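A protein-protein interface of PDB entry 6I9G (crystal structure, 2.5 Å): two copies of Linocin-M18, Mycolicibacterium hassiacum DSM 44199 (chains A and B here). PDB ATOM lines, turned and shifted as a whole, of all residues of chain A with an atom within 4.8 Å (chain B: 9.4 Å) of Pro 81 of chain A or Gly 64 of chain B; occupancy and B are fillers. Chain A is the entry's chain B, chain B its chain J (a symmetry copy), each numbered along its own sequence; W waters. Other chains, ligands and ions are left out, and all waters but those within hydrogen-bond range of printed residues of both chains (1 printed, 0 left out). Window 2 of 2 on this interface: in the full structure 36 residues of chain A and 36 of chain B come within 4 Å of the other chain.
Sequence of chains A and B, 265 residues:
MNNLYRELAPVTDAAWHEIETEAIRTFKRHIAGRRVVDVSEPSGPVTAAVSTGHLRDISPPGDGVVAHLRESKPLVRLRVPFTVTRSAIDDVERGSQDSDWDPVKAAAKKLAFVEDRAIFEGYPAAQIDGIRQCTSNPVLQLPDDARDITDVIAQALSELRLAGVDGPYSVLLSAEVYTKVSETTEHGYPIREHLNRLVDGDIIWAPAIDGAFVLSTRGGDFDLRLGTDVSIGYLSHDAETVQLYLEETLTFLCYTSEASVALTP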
ATOM      1  N   ARG A  79      27.904   9.544 -33.334  1.00  0.00           N
ATOM      2  CA  ARG A  79      28.048  10.988 -33.289  1.00  0.00           C
ATOM      3  C   ARG A  79      28.126  11.488 -31.851  1.00  0.00           C
ATOM      4  O   ARG A  79      27.317  11.106 -31.002  1.00  0.00           O
ATOM      5  CB  ARG A  79      26.892  11.652 -34.018  1.00  0.00           C
ATOM      6  CG  ARG A  79      27.029  13.157 -34.073  1.00  0.00           C
ATOM      7  CD  ARG A  79      25.876  13.784 -34.830  1.00  0.00           C
ATOM      8  NE  ARG A  79      26.054  13.738 -36.280  1.00  0.00           N
ATOM      9  CZ  ARG A  79      25.252  14.362 -37.138  1.00  0.00           C
ATOM     10  NH1 ARG A  79      24.224  15.072 -36.685  1.00  0.00           N
ATOM     11  NH2 ARG A  79      25.471  14.275 -38.439  1.00  0.00           N
ATOM     12  N   VAL A  80      29.120  12.328 -31.586  1.00  0.00           N
ATOM     13  CA  VAL A  80      29.309  12.921 -30.273  1.00  0.00           C
ATOM     14  C   VAL A  80      29.285  14.450 -30.388  1.00  0.00           C
ATOM     15  O   VAL A  80      30.304  15.062 -30.747  1.00  0.00           O
ATOM     16  CB  VAL A  80      30.623  12.464 -29.649  1.00  0.00           C
ATOM     17  CG1 VAL A  80      30.755  12.991 -28.224  1.00  0.00           C
ATOM     18  CG2 VAL A  80      30.687  10.948 -29.671  1.00  0.00           C
ATOM     19  N   PRO A  81      28.119  15.077 -30.084  1.00  0.00           N
ATOM     20  CA  PRO A  81      28.031  16.536 -30.161  1.00  0.00           C
ATOM     21  C   PRO A  81      28.819  17.163 -29.020  1.00  0.00           C
ATOM     22  O   PRO A  81      28.921  16.572 -27.948  1.00  0.00           O
ATOM     23  CB  PRO A  81      26.539  16.825 -29.961  1.00  0.00           C
ATOM     24  CG  PRO A  81      25.864  15.505 -29.930  1.00  0.00           C
ATOM     25  CD  PRO A  81      26.892  14.498 -29.517  1.00  0.00           C
ATOM     26  N   PHE A  82      29.393  18.336 -29.282  1.00  0.00           N
ATOM     27  CA  PHE A  82      30.061  19.127 -28.280  1.00  0.00           C
ATOM     28  C   PHE A  82      29.914  20.614 -28.610  1.00  0.00           C
ATOM     29  O   PHE A  82      29.680  20.996 -29.774  1.00  0.00           O
ATOM     30  CB  PHE A  82      31.536  18.707 -28.139  1.00  0.00           C
ATOM     31  CG  PHE A  82      32.377  19.010 -29.336  1.00  0.00           C
ATOM     32  CD1 PHE A  82      33.029  20.237 -29.457  1.00  0.00           C
ATOM     33  CD2 PHE A  82      32.520  18.076 -30.357  1.00  0.00           C
ATOM     34  CE1 PHE A  82      33.808  20.535 -30.576  1.00  0.00           C
ATOM     35  CE2 PHE A  82      33.315  18.353 -31.470  1.00  0.00           C
ATOM     36  CZ  PHE A  82      33.961  19.590 -31.582  1.00  0.00           C
ATOM     37  N   THR A  83      30.053  21.447 -27.575  1.00  0.00           N
ATOM     38  CA  THR A  83      29.910  22.888 -27.713  1.00  0.00           C
ATOM     39  C   THR A  83      31.163  23.602 -27.284  1.00  0.00           C
ATOM     40  O   THR A  83      31.681  23.343 -26.204  1.00  0.00           O
ATOM     41  CB  THR A  83      28.739  23.402 -26.872  1.00  0.00           C
ATOM     42  OG1 THR A  83      27.545  22.835 -27.396  1.00  0.00           O
ATOM     43  CG2 THR A  83      28.636  24.917 -26.933  1.00  0.00           C
ATOM     44  N   LYS A 110      35.172  10.314 -25.444  1.00  0.00           N
ATOM     45  CA  LYS A 110      33.875   9.654 -25.517  1.00  0.00           C
ATOM     46  C   LYS A 110      33.796   8.721 -26.728  1.00  0.00           C
ATOM     47  O   LYS A 110      33.468   7.536 -26.602  1.00  0.00           O
ATOM     48  CB  LYS A 110      32.764  10.702 -25.554  1.00  0.00           C
ATOM     49  CG  LYS A 110      31.409  10.196 -25.096  1.00  0.00           C
ATOM     50  CD  LYS A 110      31.128  10.392 -23.596  1.00  0.00           C
ATOM     51  CE  LYS A 110      30.277  11.629 -23.280  1.00  0.00           C
ATOM     52  NZ  LYS A 110      31.027  12.920 -23.339  1.00  0.00           N
ATOM     53  N   LEU A 235      26.624  21.805 -36.255  1.00  0.00           N
ATOM     54  CA  LEU A 235      25.174  21.725 -36.034  1.00  0.00           C
ATOM     55  C   LEU A 235      24.495  23.092 -36.034  1.00  0.00           C
ATOM     56  O   LEU A 235      23.608  23.349 -36.854  1.00  0.00           O
ATOM     57  CB  LEU A 235      24.836  21.008 -34.736  1.00  0.00           C
ATOM     58  CG  LEU A 235      24.869  19.482 -34.793  1.00  0.00           C
ATOM     59  CD1 LEU A 235      24.887  18.907 -33.387  1.00  0.00           C
ATOM     60  CD2 LEU A 235      23.700  18.913 -35.565  1.00  0.00           C
ATOM     61  N   GLN A 243      27.903  24.775 -31.692  1.00  0.00           N
ATOM     62  CA  GLN A 243      27.758  23.350 -31.481  1.00  0.00           C
ATOM     63  C   GLN A 243      28.239  22.562 -32.689  1.00  0.00           C
ATOM     64  O   GLN A 243      27.725  22.711 -33.806  1.00  0.00           O
ATOM     65  CB  GLN A 243      26.334  22.944 -31.105  1.00  0.00           C
ATOM     66  CG  GLN A 243      26.287  21.459 -30.749  1.00  0.00           C
ATOM     67  CD  GLN A 243      24.909  20.956 -30.353  1.00  0.00           C
ATOM     68  OE1 GLN A 243      23.888  21.432 -30.851  1.00  0.00           O
ATOM     69  NE2 GLN A 243      24.879  19.968 -29.463  1.00  0.00           N
ATOM     70  N   LEU A 244      29.239  21.723 -32.436  1.00  0.00           N
ATOM     71  CA  LEU A 244      29.813  20.855 -33.442  1.00  0.00           C
ATOM     72  C   LEU A 244      29.637  19.406 -32.981  1.00  0.00           C
ATOM     73  O   LEU A 244      28.943  19.141 -31.994  1.00  0.00           O
ATOM     74  CB  LEU A 244      31.293  21.190 -33.620  1.00  0.00           C
ATOM     75  CG  LEU A 244      31.667  22.663 -33.797  1.00  0.00           C
ATOM     76  CD1 LEU A 244      33.156  22.850 -33.560  1.00  0.00           C
ATOM     77  CD2 LEU A 244      31.285  23.141 -35.186  1.00  0.00           C
ATOM     78  N   TYR A 245      30.248  18.468 -33.699  1.00  0.00           N
ATOM     79  CA  TYR A 245      30.260  17.075 -33.287  1.00  0.00           C
ATOM     80  C   TYR A 245      31.423  16.354 -33.921  1.00  0.00           C
ATOM     81  O   TYR A 245      31.947  16.761 -34.967  1.00  0.00           O
ATOM     82  CB  TYR A 245      28.978  16.369 -33.707  1.00  0.00           C
ATOM     83  CG  TYR A 245      28.697  16.465 -35.196  1.00  0.00           C
ATOM     84  CD1 TYR A 245      29.364  15.651 -36.122  1.00  0.00           C
ATOM     85  CD2 TYR A 245      27.768  17.369 -35.677  1.00  0.00           C
ATOM     86  CE1 TYR A 245      29.100  15.745 -37.478  1.00  0.00           C
ATOM     87  CE2 TYR A 245      27.489  17.469 -37.033  1.00  0.00           C
ATOM     88  CZ  TYR A 245      28.148  16.658 -37.935  1.00  0.00           C
ATOM     89  OH  TYR A 245      27.865  16.796 -39.288  1.00  0.00           O
ATOM     90  N   PRO B  60      21.552   4.450 -27.873  1.00  0.00           N
ATOM     91  CA  PRO B  60      22.920   4.946 -27.839  1.00  0.00           C
ATOM     92  C   PRO B  60      23.810   4.010 -27.069  1.00  0.00           C
ATOM     93  O   PRO B  60      23.309   3.246 -26.259  1.00  0.00           O
ATOM     94  CB  PRO B  60      22.795   6.262 -27.077  1.00  0.00           C
ATOM     95  CG  PRO B  60      21.554   6.122 -26.273  1.00  0.00           C
ATOM     96  CD  PRO B  60      20.631   5.331 -27.134  1.00  0.00           C
ATOM     97  N   PRO B  61      25.128   4.068 -27.307  1.00  0.00           N
ATOM     98  CA  PRO B  61      26.056   3.234 -26.553  1.00  0.00           C
ATOM     99  C   PRO B  61      26.527   3.857 -25.239  1.00  0.00           C
ATOM    100  O   PRO B  61      27.380   3.272 -24.590  1.00  0.00           O
ATOM    101  CB  PRO B  61      27.245   3.131 -27.495  1.00  0.00           C
ATOM    102  CG  PRO B  61      27.272   4.472 -28.141  1.00  0.00           C
ATOM    103  CD  PRO B  61      25.823   4.822 -28.367  1.00  0.00           C
ATOM    104  N   GLY B  62      26.010   5.022 -24.857  1.00  0.00           N
ATOM    105  CA  GLY B  62      26.488   5.734 -23.657  1.00  0.00           C
ATOM    106  C   GLY B  62      26.038   7.176 -23.717  1.00  0.00           C
ATOM    107  O   GLY B  62      25.558   7.614 -24.750  1.00  0.00           O
ATOM    108  N   ASP B  63      26.187   7.932 -22.638  1.00  0.00           N
ATOM    109  CA  ASP B  63      25.652   9.300 -22.618  1.00  0.00           C
ATOM    110  C   ASP B  63      26.423  10.211 -23.544  1.00  0.00           C
ATOM    111  O   ASP B  63      27.641  10.084 -23.677  1.00  0.00           O
ATOM    112  CB  ASP B  63      25.670   9.899 -21.205  1.00  0.00           C
ATOM    113  CG  ASP B  63      24.811   9.122 -20.226  1.00  0.00           C
ATOM    114  OD1 ASP B  63      23.725   8.633 -20.618  1.00  0.00           O
ATOM    115  OD2 ASP B  63      25.230   8.997 -19.056  1.00  0.00           O
ATOM    116  N   GLY B  64      25.706  11.133 -24.174  1.00  0.00           N
ATOM    117  CA  GLY B  64      26.315  12.119 -25.045  1.00  0.00           C
ATOM    118  C   GLY B  64      26.721  11.539 -26.379  1.00  0.00           C
ATOM    119  O   GLY B  64      27.420  12.195 -27.145  1.00  0.00           O
ATOM    120  N   VAL B  65      26.291  10.311 -26.659  1.00  0.00           N
ATOM    121  CA  VAL B  65      26.517   9.710 -27.964  1.00  0.00           C
ATOM    122  C   VAL B  65      25.194   9.412 -28.636  1.00  0.00           C
ATOM    123  O   VAL B  65      24.270   8.896 -28.035  1.00  0.00           O
ATOM    124  CB  VAL B  65      27.339   8.417 -27.878  1.00  0.00           C
ATOM    125  CG1 VAL B  65      27.657   7.898 -29.277  1.00  0.00           C
ATOM    126  CG2 VAL B  65      28.618   8.664 -27.097  1.00  0.00           C
ATOM    127  N   VAL B  66      25.106   9.746 -29.902  1.00  0.00           N
ATOM    128  CA  VAL B  66      23.897   9.512 -30.649  1.00  0.00           C
ATOM    129  C   VAL B  66      24.263   8.516 -31.739  1.00  0.00           C
ATOM    130  O   VAL B  66      25.201   8.763 -32.480  1.00  0.00           O
ATOM    131  CB  VAL B  66      23.407  10.851 -31.230  1.00  0.00           C
ATOM    132  CG1 VAL B  66      22.376  10.645 -32.326  1.00  0.00           C
ATOM    133  CG2 VAL B  66      22.840  11.711 -30.110  1.00  0.00           C
ATOM    134  N   ALA B  67      23.557   7.392 -31.831  1.00  0.00           N
ATOM    135  CA  ALA B  67      23.922   6.354 -32.797  1.00  0.00           C
ATOM    136  C   ALA B  67      22.802   6.080 -33.806  1.00  0.00           C
ATOM    137  O   ALA B  67      21.631   6.088 -33.431  1.00  0.00           O
ATOM    138  CB  ALA B  67      24.299   5.081 -32.071  1.00  0.00           C
HETATM  139  O   HOH W   1      28.213  14.520 -26.548  1.00  0.00           O
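The backbone NH (N) of Val 66 of chain B is in hydrogen-bond range of the backbone carbonyl oxygen (O) of Arg 79 of chain A (2.8 Å).
Among the printed residues, pairs that only touch across the chains: Arg 79 of chain A with Val 65 of chain B, Val 80 of chain A with Gly 64 of chain B, Pro 81 of chain A with Gly 64 of chain B, Lys 110 of chain A with Asp 63 of chain B and Lys 110 of chain A with Val 65 of chain B.
Of the printed residues of chain A, Gly 64 of chain B touches Val 80 (3.6 Å) and Pro 81 (3.3 Å).
Printed residues of chain B within 4 Å of Arg 79 of chain A: Val 65 and Val 66.
Printed residues of chain B within 4 Å of Lys 110 of chain A: Asp 63 (3.1 Å) and Val 65 (3.8 Å).
Gly 62 of chain B touches none of the printed residues of chain A.
Pro 61 of chain B touches none of the printed residues of chain A.
The nearest printed residue of chain B that does not touch Lys 110 of chain A is Gly 64 of chain B (4.4 Å).
Printed residues of chain A that touch a printed residue of chain B: Arg 79, Val 80, Pro 81 and Lys 110.
Hydrophobic or aromatic side chains of chain A within 4 Å of the printed part of chain B: Val 80 and Pro 81.
Among the printed residues, no Asp or Glu carboxylate lies within 4 Å of a Lys or Arg side-chain nitrogen of the other chain.
No position is printed for both chains.
Of the 6 pairs that touch across the chains among the printed residues, none has its exchanged pair printed and touching as well.
Water W1 bridges the backbone carbonyl oxygen (O) of Gly 64 of chain B (2.5 Å) and the backbone carbonyl oxygen (O) of Pro 81 of chain A (2.6 Å).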
